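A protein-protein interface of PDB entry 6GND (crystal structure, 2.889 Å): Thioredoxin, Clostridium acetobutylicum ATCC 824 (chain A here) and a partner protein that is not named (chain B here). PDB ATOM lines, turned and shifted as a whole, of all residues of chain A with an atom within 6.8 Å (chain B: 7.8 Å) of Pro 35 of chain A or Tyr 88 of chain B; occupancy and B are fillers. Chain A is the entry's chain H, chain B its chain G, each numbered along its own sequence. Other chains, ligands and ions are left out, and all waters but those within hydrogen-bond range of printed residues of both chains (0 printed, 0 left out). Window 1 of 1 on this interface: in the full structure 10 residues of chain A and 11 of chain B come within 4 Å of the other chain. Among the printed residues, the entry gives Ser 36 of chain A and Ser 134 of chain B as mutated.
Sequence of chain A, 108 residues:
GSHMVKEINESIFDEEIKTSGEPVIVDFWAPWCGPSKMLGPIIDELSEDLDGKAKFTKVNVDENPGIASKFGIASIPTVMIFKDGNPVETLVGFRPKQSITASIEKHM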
ATOM      1  N   ALA A  30     -35.213   2.192  -7.799  1.00  0.00           N
ATOM      2  CA  ALA A  30     -34.864   2.279  -9.209  1.00  0.00           C
ATOM      3  C   ALA A  30     -33.555   1.548  -9.459  1.00  0.00           C
ATOM      4  O   ALA A  30     -32.699   1.484  -8.569  1.00  0.00           O
ATOM      5  CB  ALA A  30     -34.736   3.745  -9.655  1.00  0.00           C
ATOM      6  N   TRP A  32     -30.976   2.369 -11.289  1.00  0.00           N
ATOM      7  CA  TRP A  32     -29.787   3.202 -11.416  1.00  0.00           C
ATOM      8  C   TRP A  32     -29.298   3.736 -10.075  1.00  0.00           C
ATOM      9  O   TRP A  32     -28.106   4.044  -9.941  1.00  0.00           O
ATOM     10  CB  TRP A  32     -30.071   4.357 -12.388  1.00  0.00           C
ATOM     11  CG  TRP A  32     -31.136   5.287 -11.928  1.00  0.00           C
ATOM     12  CD1 TRP A  32     -30.986   6.371 -11.115  1.00  0.00           C
ATOM     13  CD2 TRP A  32     -32.536   5.187 -12.211  1.00  0.00           C
ATOM     14  NE1 TRP A  32     -32.203   6.973 -10.899  1.00  0.00           N
ATOM     15  CE2 TRP A  32     -33.172   6.260 -11.555  1.00  0.00           C
ATOM     16  CE3 TRP A  32     -33.312   4.299 -12.960  1.00  0.00           C
ATOM     17  CZ2 TRP A  32     -34.547   6.468 -11.627  1.00  0.00           C
ATOM     18  CZ3 TRP A  32     -34.676   4.509 -13.034  1.00  0.00           C
ATOM     19  CH2 TRP A  32     -35.280   5.585 -12.372  1.00  0.00           C
ATOM     20  N   CYS A  33     -30.179   3.836  -9.083  1.00  0.00           N
ATOM     21  CA  CYS A  33     -29.842   4.400  -7.780  1.00  0.00           C
ATOM     22  C   CYS A  33     -29.242   3.339  -6.858  1.00  0.00           C
ATOM     23  O   CYS A  33     -29.894   2.337  -6.544  1.00  0.00           O
ATOM     24  CB  CYS A  33     -31.087   5.008  -7.133  1.00  0.00           C
ATOM     25  SG  CYS A  33     -30.746   6.138  -5.756  1.00  0.00           S
ATOM     26  N   GLY A  34     -27.999   3.563  -6.432  1.00  0.00           N
ATOM     27  CA  GLY A  34     -27.327   2.668  -5.521  1.00  0.00           C
ATOM     28  C   GLY A  34     -28.036   2.572  -4.183  1.00  0.00           C
ATOM     29  O   GLY A  34     -28.321   1.479  -3.683  1.00  0.00           O
ATOM     30  N   PRO A  35     -28.323   3.723  -3.567  1.00  0.00           N
ATOM     31  CA  PRO A  35     -29.083   3.701  -2.303  1.00  0.00           C
ATOM     32  C   PRO A  35     -30.362   2.886  -2.380  1.00  0.00           C
ATOM     33  O   PRO A  35     -30.637   2.081  -1.479  1.00  0.00           O
ATOM     34  CB  PRO A  35     -29.359   5.188  -2.044  1.00  0.00           C
ATOM     35  CG  PRO A  35     -28.218   5.890  -2.688  1.00  0.00           C
ATOM     36  CD  PRO A  35     -27.852   5.079  -3.904  1.00  0.00           C
ATOM     37  N   SER A  36     -31.164   3.081  -3.428  1.00  0.00           N
ATOM     38  CA  SER A  36     -32.391   2.307  -3.568  1.00  0.00           C
ATOM     39  C   SER A  36     -32.098   0.818  -3.633  1.00  0.00           C
ATOM     40  O   SER A  36     -32.882   0.003  -3.134  1.00  0.00           O
ATOM     41  CB  SER A  36     -33.158   2.740  -4.813  1.00  0.00           C
ATOM     42  OG  SER A  36     -32.462   2.361  -5.987  1.00  0.00           O
ATOM     43  N   LYS A  37     -30.976   0.446  -4.254  1.00  0.00           N
ATOM     44  CA  LYS A  37     -30.562  -0.951  -4.259  1.00  0.00           C
ATOM     45  C   LYS A  37     -30.332  -1.446  -2.840  1.00  0.00           C
ATOM     46  O   LYS A  37     -30.858  -2.489  -2.440  1.00  0.00           O
ATOM     47  CB  LYS A  37     -29.300  -1.120  -5.105  1.00  0.00           C
ATOM     48  N   MET A  38     -29.541  -0.712  -2.059  1.00  0.00           N
ATOM     49  CA  MET A  38     -29.298  -1.112  -0.679  1.00  0.00           C
ATOM     50  C   MET A  38     -30.610  -1.260   0.083  1.00  0.00           C
ATOM     51  O   MET A  38     -30.776  -2.181   0.889  1.00  0.00           O
ATOM     52  CB  MET A  38     -28.403  -0.091   0.019  1.00  0.00           C
ATOM     53  CG  MET A  38     -27.130   0.296  -0.732  1.00  0.00           C
ATOM     54  SD  MET A  38     -26.088  -1.080  -1.253  1.00  0.00           S
ATOM     55  CE  MET A  38     -24.741  -0.191  -2.027  1.00  0.00           C
ATOM     56  N   LEU A  39     -31.554  -0.346  -0.161  1.00  0.00           N
ATOM     57  CA  LEU A  39     -32.821  -0.361   0.562  1.00  0.00           C
ATOM     58  C   LEU A  39     -33.603  -1.642   0.299  1.00  0.00           C
ATOM     59  O   LEU A  39     -34.230  -2.190   1.214  1.00  0.00           O
ATOM     60  CB  LEU A  39     -33.645   0.865   0.163  1.00  0.00           C
ATOM     61  CG  LEU A  39     -33.839   1.966   1.206  1.00  0.00           C
ATOM     62  CD1 LEU A  39     -34.781   3.027   0.659  1.00  0.00           C
ATOM     63  CD2 LEU A  39     -34.379   1.405   2.514  1.00  0.00           C
ATOM     64  N   GLY A  40     -33.586  -2.131  -0.941  1.00  0.00           N
ATOM     65  CA  GLY A  40     -34.344  -3.306  -1.310  1.00  0.00           C
ATOM     66  C   GLY A  40     -34.080  -4.475  -0.383  1.00  0.00           C
ATOM     67  O   GLY A  40     -34.921  -4.860   0.435  1.00  0.00           O
ATOM     68  N   PRO A  77     -35.039   6.869  -3.554  1.00  0.00           N
ATOM     69  CA  PRO A  77     -35.172   5.912  -2.451  1.00  0.00           C
ATOM     70  C   PRO A  77     -36.143   6.433  -1.406  1.00  0.00           C
ATOM     71  O   PRO A  77     -35.742   7.112  -0.455  1.00  0.00           O
ATOM     72  CB  PRO A  77     -33.743   5.806  -1.912  1.00  0.00           C
ATOM     73  CG  PRO A  77     -33.162   7.169  -2.167  1.00  0.00           C
ATOM     74  CD  PRO A  77     -33.875   7.758  -3.372  1.00  0.00           C
ATOM     75  N   GLY A  93     -35.014   8.848   1.150  1.00  0.00           N
ATOM     76  CA  GLY A  93     -33.612   8.561   1.352  1.00  0.00           C
ATOM     77  C   GLY A  93     -33.404   7.238   2.068  1.00  0.00           C
ATOM     78  O   GLY A  93     -34.298   6.696   2.717  1.00  0.00           O
ATOM     79  N   PHE A  94     -32.189   6.713   1.941  1.00  0.00           N
ATOM     80  CA  PHE A  94     -31.848   5.466   2.612  1.00  0.00           C
ATOM     81  C   PHE A  94     -32.004   5.615   4.119  1.00  0.00           C
ATOM     82  O   PHE A  94     -31.700   6.664   4.694  1.00  0.00           O
ATOM     83  CB  PHE A  94     -30.419   5.048   2.263  1.00  0.00           C
ATOM     84  CG  PHE A  94     -29.978   3.773   2.930  1.00  0.00           C
ATOM     85  CD1 PHE A  94     -29.541   3.775   4.245  1.00  0.00           C
ATOM     86  CD2 PHE A  94     -30.006   2.570   2.245  1.00  0.00           C
ATOM     87  CE1 PHE A  94     -29.138   2.609   4.861  1.00  0.00           C
ATOM     88  CE2 PHE A  94     -29.604   1.398   2.859  1.00  0.00           C
ATOM     89  CZ  PHE A  94     -29.170   1.420   4.168  1.00  0.00           C
ATOM     90  N   PRO A  96     -31.493   2.999   7.817  1.00  0.00           N
ATOM     91  CA  PRO A  96     -31.068   1.688   8.318  1.00  0.00           C
ATOM     92  C   PRO A  96     -32.244   0.885   8.859  1.00  0.00           C
ATOM     93  O   PRO A  96     -33.338   1.399   9.093  1.00  0.00           O
ATOM     94  CB  PRO A  96     -30.071   2.042   9.427  1.00  0.00           C
ATOM     95  CG  PRO A  96     -30.524   3.369   9.919  1.00  0.00           C
ATOM     96  CD  PRO A  96     -31.094   4.092   8.725  1.00  0.00           C
ATOM     97  N   ASN B  85     -17.384   8.795   0.382  1.00  0.00           N
ATOM     98  CA  ASN B  85     -18.617   9.448  -0.028  1.00  0.00           C
ATOM     99  C   ASN B  85     -19.833   8.977   0.768  1.00  0.00           C
ATOM    100  O   ASN B  85     -20.684   9.801   1.125  1.00  0.00           O
ATOM    101  CB  ASN B  85     -18.837   9.230  -1.532  1.00  0.00           C
ATOM    102  CG  ASN B  85     -17.732   9.852  -2.376  1.00  0.00           C
ATOM    103  OD1 ASN B  85     -17.258  10.951  -2.084  1.00  0.00           O
ATOM    104  ND2 ASN B  85     -17.320   9.152  -3.428  1.00  0.00           N
ATOM    105  N   ASN B  86     -19.945   7.682   1.069  1.00  0.00           N
ATOM    106  CA  ASN B  86     -21.130   7.188   1.766  1.00  0.00           C
ATOM    107  C   ASN B  86     -20.838   5.906   2.534  1.00  0.00           C
ATOM    108  O   ASN B  86     -19.907   5.164   2.217  1.00  0.00           O
ATOM    109  CB  ASN B  86     -22.291   6.961   0.793  1.00  0.00           C
ATOM    110  CG  ASN B  86     -23.065   8.230   0.504  1.00  0.00           C
ATOM    111  OD1 ASN B  86     -23.218   9.089   1.378  1.00  0.00           O
ATOM    112  ND2 ASN B  86     -23.551   8.363  -0.727  1.00  0.00           N
ATOM    113  N   ILE B  87     -21.664   5.665   3.556  1.00  0.00           N
ATOM    114  CA  ILE B  87     -21.569   4.482   4.411  1.00  0.00           C
ATOM    115  C   ILE B  87     -22.980   4.010   4.744  1.00  0.00           C
ATOM    116  O   ILE B  87     -23.730   4.728   5.416  1.00  0.00           O
ATOM    117  CB  ILE B  87     -20.798   4.778   5.710  1.00  0.00           C
ATOM    118  CG1 ILE B  87     -19.411   5.341   5.395  1.00  0.00           C
ATOM    119  CG2 ILE B  87     -20.701   3.515   6.556  1.00  0.00           C
ATOM    120  CD1 ILE B  87     -18.672   5.865   6.606  1.00  0.00           C
ATOM    121  N   TYR B  88     -23.339   2.804   4.297  1.00  0.00           N
ATOM    122  CA  TYR B  88     -24.691   2.265   4.446  1.00  0.00           C
ATOM    123  C   TYR B  88     -24.703   1.148   5.485  1.00  0.00           C
ATOM    124  O   TYR B  88     -24.069   0.105   5.286  1.00  0.00           O
ATOM    125  CB  TYR B  88     -25.223   1.740   3.109  1.00  0.00           C
ATOM    126  CG  TYR B  88     -25.279   2.778   2.011  1.00  0.00           C
ATOM    127  CD1 TYR B  88     -24.140   3.124   1.297  1.00  0.00           C
ATOM    128  CD2 TYR B  88     -26.473   3.404   1.682  1.00  0.00           C
ATOM    129  CE1 TYR B  88     -24.188   4.068   0.294  1.00  0.00           C
ATOM    130  CE2 TYR B  88     -26.529   4.351   0.679  1.00  0.00           C
ATOM    131  CZ  TYR B  88     -25.383   4.677  -0.011  1.00  0.00           C
ATOM    132  OH  TYR B  88     -25.428   5.618  -1.012  1.00  0.00           O
ATOM    133  N   ALA B  89     -25.426   1.365   6.585  1.00  0.00           N
ATOM    134  CA  ALA B  89     -25.520   0.382   7.667  1.00  0.00           C
ATOM    135  C   ALA B  89     -26.514  -0.708   7.278  1.00  0.00           C
ATOM    136  O   ALA B  89     -27.729  -0.506   7.335  1.00  0.00           O
ATOM    137  CB  ALA B  89     -25.938   1.063   8.966  1.00  0.00           C
ATOM    138  N   MET B  90     -25.999  -1.879   6.898  1.00  0.00           N
ATOM    139  CA  MET B  90     -26.845  -2.982   6.456  1.00  0.00           C
ATOM    140  C   MET B  90     -27.357  -3.861   7.592  1.00  0.00           C
ATOM    141  O   MET B  90     -28.338  -4.586   7.394  1.00  0.00           O
ATOM    142  CB  MET B  90     -26.090  -3.855   5.451  1.00  0.00           C
ATOM    143  CG  MET B  90     -25.619  -3.089   4.238  1.00  0.00           C
ATOM    144  SD  MET B  90     -26.984  -2.265   3.400  1.00  0.00           S
ATOM    145  CE  MET B  90     -26.119  -1.655   1.964  1.00  0.00           C
ATOM    146  N   GLY B  91     -26.715  -3.835   8.757  1.00  0.00           N
ATOM    147  CA  GLY B  91     -27.157  -4.645   9.875  1.00  0.00           C
ATOM    148  C   GLY B  91     -26.029  -5.440  10.493  1.00  0.00           C
ATOM    149  O   GLY B  91     -25.634  -5.185  11.636  1.00  0.00           O
ATOM    150  N   TYR B  93     -23.044  -5.597   8.833  1.00  0.00           N
ATOM    151  CA  TYR B  93     -21.818  -4.974   8.362  1.00  0.00           C
ATOM    152  C   TYR B  93     -22.137  -3.582   7.833  1.00  0.00           C
ATOM    153  O   TYR B  93     -23.294  -3.150   7.813  1.00  0.00           O
ATOM    154  CB  TYR B  93     -21.152  -5.812   7.269  1.00  0.00           C
ATOM    155  CG  TYR B  93     -21.896  -5.777   5.954  1.00  0.00           C
ATOM    156  CD1 TYR B  93     -23.053  -6.520   5.763  1.00  0.00           C
ATOM    157  CD2 TYR B  93     -21.444  -4.989   4.904  1.00  0.00           C
ATOM    158  CE1 TYR B  93     -23.735  -6.482   4.559  1.00  0.00           C
ATOM    159  CE2 TYR B  93     -22.119  -4.946   3.702  1.00  0.00           C
ATOM    160  CZ  TYR B  93     -23.261  -5.694   3.533  1.00  0.00           C
ATOM    161  OH  TYR B  93     -23.930  -5.649   2.333  1.00  0.00           O
ATOM    162  N   PHE B  94     -21.092  -2.884   7.397  1.00  0.00           N
ATOM    163  CA  PHE B  94     -21.209  -1.554   6.816  1.00  0.00           C
ATOM    164  C   PHE B  94     -20.595  -1.576   5.429  1.00  0.00           C
ATOM    165  O   PHE B  94     -19.455  -2.019   5.259  1.00  0.00           O
ATOM    166  CB  PHE B  94     -20.512  -0.504   7.676  1.00  0.00           C
ATOM    167  CG  PHE B  94     -21.116  -0.357   9.025  1.00  0.00           C
ATOM    168  CD1 PHE B  94     -22.188   0.490   9.223  1.00  0.00           C
ATOM    169  CD2 PHE B  94     -20.630  -1.085  10.095  1.00  0.00           C
ATOM    170  CE1 PHE B  94     -22.759   0.620  10.465  1.00  0.00           C
ATOM    171  CE2 PHE B  94     -21.194  -0.957  11.340  1.00  0.00           C
ATOM    172  CZ  PHE B  94     -22.264  -0.104  11.527  1.00  0.00           C
ATOM    173  N   SER B  95     -21.346  -1.101   4.446  1.00  0.00           N
ATOM    174  CA  SER B  95     -20.845  -0.968   3.088  1.00  0.00           C
ATOM    175  C   SER B  95     -20.335   0.452   2.903  1.00  0.00           C
ATOM    176  O   SER B  95     -21.057   1.421   3.172  1.00  0.00           O
ATOM    177  CB  SER B  95     -21.928  -1.296   2.064  1.00  0.00           C
ATOM    178  OG  SER B  95     -22.308  -2.661   2.156  1.00  0.00           O
ATOM    179  N   ILE B  96     -19.095   0.569   2.447  1.00  0.00           N
ATOM    180  CA  ILE B  96     -18.402   1.846   2.358  1.00  0.00           C
ATOM    181  C   ILE B  96     -18.190   2.158   0.885  1.00  0.00           C
ATOM    182  O   ILE B  96     -17.480   1.429   0.180  1.00  0.00           O
ATOM    183  CB  ILE B  96     -17.077   1.810   3.132  1.00  0.00           C
ATOM    184  CG1 ILE B  96     -17.358   1.456   4.594  1.00  0.00           C
ATOM    185  CG2 ILE B  96     -16.370   3.150   3.029  1.00  0.00           C
ATOM    186  CD1 ILE B  96     -16.128   1.162   5.412  1.00  0.00           C
ATOM    187  N   MET B  97     -18.809   3.239   0.425  1.00  0.00           N
ATOM    188  CA  MET B  97     -18.768   3.639  -0.972  1.00  0.00           C
ATOM    189  C   MET B  97     -17.737   4.740  -1.167  1.00  0.00           C
ATOM    190  O   MET B  97     -17.696   5.705  -0.395  1.00  0.00           O
ATOM    191  CB  MET B  97     -20.134   4.138  -1.450  1.00  0.00           C
ATOM    192  CG  MET B  97     -21.282   3.176  -1.233  1.00  0.00           C
ATOM    193  SD  MET B  97     -21.120   1.650  -2.170  1.00  0.00           S
ATOM    194  CE  MET B  97     -21.064   0.462  -0.833  1.00  0.00           C
ATOM    195  N   THR B  98     -16.899   4.578  -2.181  1.00  0.00           N
ATOM    196  CA  THR B  98     -16.068   5.655  -2.689  1.00  0.00           C
ATOM    197  C   THR B  98     -16.208   5.669  -4.204  1.00  0.00           C
ATOM    198  O   THR B  98     -16.660   4.697  -4.814  1.00  0.00           O
ATOM    199  CB  THR B  98     -14.594   5.498  -2.296  1.00  0.00           C
ATOM    200  OG1 THR B  98     -13.997   4.445  -3.062  1.00  0.00           O
ATOM    201  CG2 THR B  98     -14.466   5.180  -0.816  1.00  0.00           C
ATOM    202  N   TYR B 103     -16.043  -0.868  -0.341  1.00  0.00           N
ATOM    203  CA  TYR B 103     -15.484  -1.644   0.764  1.00  0.00           C
ATOM    204  C   TYR B 103     -16.557  -2.006   1.789  1.00  0.00           C
ATOM    205  O   TYR B 103     -17.542  -1.286   1.936  1.00  0.00           O
ATOM    206  CB  TYR B 103     -14.402  -0.846   1.483  1.00  0.00           C
ATOM    207  CG  TYR B 103     -13.321  -0.295   0.592  1.00  0.00           C
ATOM    208  CD1 TYR B 103     -13.477   0.921  -0.046  1.00  0.00           C
ATOM    209  CD2 TYR B 103     -12.133  -0.982   0.412  1.00  0.00           C
ATOM    210  CE1 TYR B 103     -12.483   1.435  -0.852  1.00  0.00           C
ATOM    211  CE2 TYR B 103     -11.133  -0.477  -0.392  1.00  0.00           C
ATOM    212  CZ  TYR B 103     -11.314   0.730  -1.020  1.00  0.00           C
ATOM    213  OH  TYR B 103     -10.318   1.235  -1.821  1.00  0.00           O
ATOM    214  N   ALA B 105     -17.106  -3.338   5.967  1.00  0.00           N
ATOM    215  CA  ALA B 105     -16.462  -3.575   7.256  1.00  0.00           C
ATOM    216  C   ALA B 105     -17.488  -3.868   8.354  1.00  0.00           C
ATOM    217  O   ALA B 105     -18.602  -3.360   8.310  1.00  0.00           O
ATOM    218  CB  ALA B 105     -15.614  -2.379   7.640  1.00  0.00           C
ATOM    219  N   VAL B 108     -17.485   0.519  12.193  1.00  0.00           N
ATOM    220  CA  VAL B 108     -17.085   1.788  11.601  1.00  0.00           C
ATOM    221  C   VAL B 108     -16.791   2.780  12.714  1.00  0.00           C
ATOM    222  O   VAL B 108     -17.445   2.766  13.763  1.00  0.00           O
ATOM    223  CB  VAL B 108     -18.172   2.358  10.662  1.00  0.00           C
ATOM    224  CG1 VAL B 108     -17.831   3.789  10.271  1.00  0.00           C
ATOM    225  CG2 VAL B 108     -18.313   1.491   9.424  1.00  0.00           C
ATOM    226  N   SER B 134     -28.270  13.735  -4.394  1.00  0.00           N
ATOM    227  CA  SER B 134     -28.432  12.537  -5.209  1.00  0.00           C
ATOM    228  C   SER B 134     -29.077  12.879  -6.543  1.00  0.00           C
ATOM    229  O   SER B 134     -30.110  12.311  -6.914  1.00  0.00           O
ATOM    230  CB  SER B 134     -29.287  11.505  -4.473  1.00  0.00           C
ATOM    231  N   CYS B 137     -29.327   9.835  -8.887  1.00  0.00           N
ATOM    232  CA  CYS B 137     -30.410   8.964  -8.465  1.00  0.00           C
ATOM    233  C   CYS B 137     -31.816   9.521  -8.744  1.00  0.00           C
ATOM    234  O   CYS B 137     -32.692   8.762  -9.151  1.00  0.00           O
ATOM    235  CB  CYS B 137     -30.269   8.634  -6.977  1.00  0.00           C
ATOM    236  SG  CYS B 137     -31.081   7.096  -6.484  1.00  0.00           S
ATOM    237  N   GLN B 228     -25.448  13.292   6.139  1.00  0.00           N
ATOM    238  CA  GLN B 228     -25.570  12.802   4.770  1.00  0.00           C
ATOM    239  C   GLN B 228     -24.592  11.668   4.493  1.00  0.00           C
ATOM    240  O   GLN B 228     -24.945  10.684   3.831  1.00  0.00           O
ATOM    241  CB  GLN B 228     -25.346  13.947   3.780  1.00  0.00           C
ATOM    242  N   LEU B 229     -23.362  11.789   4.995  1.00  0.00           N
ATOM    243  CA  LEU B 229     -22.356  10.761   4.764  1.00  0.00           C
ATOM    244  C   LEU B 229     -22.874   9.398   5.191  1.00  0.00           C
ATOM    245  O   LEU B 229     -22.701   8.403   4.479  1.00  0.00           O
ATOM    246  CB  LEU B 229     -21.085  11.102   5.541  1.00  0.00           C
ATOM    247  CG  LEU B 229     -19.921  10.115   5.463  1.00  0.00           C
ATOM    248  CD1 LEU B 229     -19.527   9.890   4.012  1.00  0.00           C
ATOM    249  CD2 LEU B 229     -18.749  10.605   6.291  1.00  0.00           C
ATOM    250  N   VAL B 230     -23.514   9.338   6.352  1.00  0.00           N
ATOM    251  CA  VAL B 230     -24.076   8.112   6.897  1.00  0.00           C
ATOM    252  C   VAL B 230     -25.588   8.276   6.973  1.00  0.00           C
ATOM    253  O   VAL B 230     -26.111   8.875   7.913  1.00  0.00           O
ATOM    254  CB  VAL B 230     -23.484   7.802   8.285  1.00  0.00           C
ATOM    255  CG1 VAL B 230     -24.069   6.511   8.840  1.00  0.00           C
ATOM    256  CG2 VAL B 230     -21.964   7.750   8.209  1.00  0.00           C
ATOM    257  N   PRO B 231     -26.330   7.761   5.994  1.00  0.00           N
ATOM    258  CA  PRO B 231     -27.794   7.862   6.061  1.00  0.00           C
ATOM    259  C   PRO B 231     -28.326   7.282   7.363  1.00  0.00           C
ATOM    260  O   PRO B 231     -27.958   6.179   7.767  1.00  0.00           O
ATOM    261  CB  PRO B 231     -28.261   7.048   4.848  1.00  0.00           C
ATOM    262  CG  PRO B 231     -27.108   7.053   3.912  1.00  0.00           C
ATOM    263  CD  PRO B 231     -25.885   7.046   4.782  1.00  0.00           C
ATOM    264  N   ILE B 250     -26.796   4.206  15.554  1.00  0.00           N
ATOM    265  CA  ILE B 250     -26.570   2.979  14.799  1.00  0.00           C
ATOM    266  C   ILE B 250     -25.871   1.979  15.711  1.00  0.00           C
ATOM    267  O   ILE B 250     -24.894   2.317  16.389  1.00  0.00           O
ATOM    268  CB  ILE B 250     -25.742   3.265  13.536  1.00  0.00           C
ATOM    269  CG1 ILE B 250     -26.460   4.310  12.676  1.00  0.00           C
ATOM    270  CG2 ILE B 250     -25.505   1.974  12.760  1.00  0.00           C
ATOM    271  CD1 ILE B 250     -25.813   4.564  11.337  1.00  0.00           C
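CG of Pro 35 of chain A touches OH of Tyr 88 of chain B, 3.3 Å away. Tyr 88 of chain B touches Met 38 of chain A (CD2 to CG, 3.99 Å). Met 90 of chain B touches Met 38 of chain A (CE to SD, 3.3 Å). CE of Met 97 of chain B touches CE of Met 38 of chain A, 3.9 Å away. CD2 of Tyr 88 of chain B touches CD2 of Phe 94 of chain A, 3.7 Å away. O of Ala 89 of chain B touches CZ of Phe 94 of chain A, at 3.98 Å. Pro 231 of chain B touches Phe 94 of chain A (CB to O, 3.5 Å). Pro 231 of chain B touches Pro 96 of chain A (O to CD, 3.9 Å).
The backbone NH (N) of Asn 85 of chain B lies within hydrogen-bond range of the backbone carbonyl oxygen (O) of Met 97 of chain B. The side-chain hydroxyl of Tyr 88 of chain B is in hydrogen-bond range of the side-chain amide nitrogen of Asn 86 of chain B, at 3.3 Å. The backbone carbonyl oxygen (O) of Asn 86 of chain B sits at hydrogen-bond distance from the backbone NH (N) of Met 97 of chain B, 2.8 Å away. The backbone carbonyl oxygen (O) of Ser 95 of chain B sits at hydrogen-bond distance from the backbone NH (N) of Tyr 88 of chain B, 2.9 Å away. The side-chain hydroxyl of Ser 36 of chain A sits at hydrogen-bond distance from O of Cys 33 of chain A (2.6 Å).
O of Cys 137 of chain B sits at hydrogen-bond distance from the indole nitrogen (NE1) of Trp 32 of chain A (2.5 Å). SG of Cys 33 of chain A is disulfide-bonded to SG of Cys 137 of chain B.
Of the printed residues of chain B, Trp 32 of chain A touches Cys 137 (2.5 Å). Pro 35 of chain A touches just one residue of chain B: Tyr 88 (3.3 Å). Of the printed residues of chain A, Tyr 88 of chain B touches Pro 35, Met 38 and Phe 94. Of the printed residues of chain A, Met 97 of chain B touches Met 38 (3.9 Å). Printed residues of chain A within 4 Å of Pro 231 of chain B: Phe 94 and Pro 96. The nearest printed residue of chain A that does not touch Ala 89 of chain B is Pro 96 of chain A (4.04 Å).
Of the 23 printed residues of chain B, 6 touch a printed residue of chain A. Hydrophobic or aromatic side chains of chain B within 4 Å of the printed part of chain A: Tyr 88, Met 90, Met 97 and Pro 231. Hydrophobic or aromatic side chains of chain A within 4 Å of the printed part of chain B: Trp 32, Pro 35, Met 38, Phe 94 and Pro 96. Among the printed residues, 10 pairs touch across the chains. Among the printed residues, no Asp or Glu carboxylate lies within 4 Å of a Lys or Arg side-chain nitrogen of the other chain.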
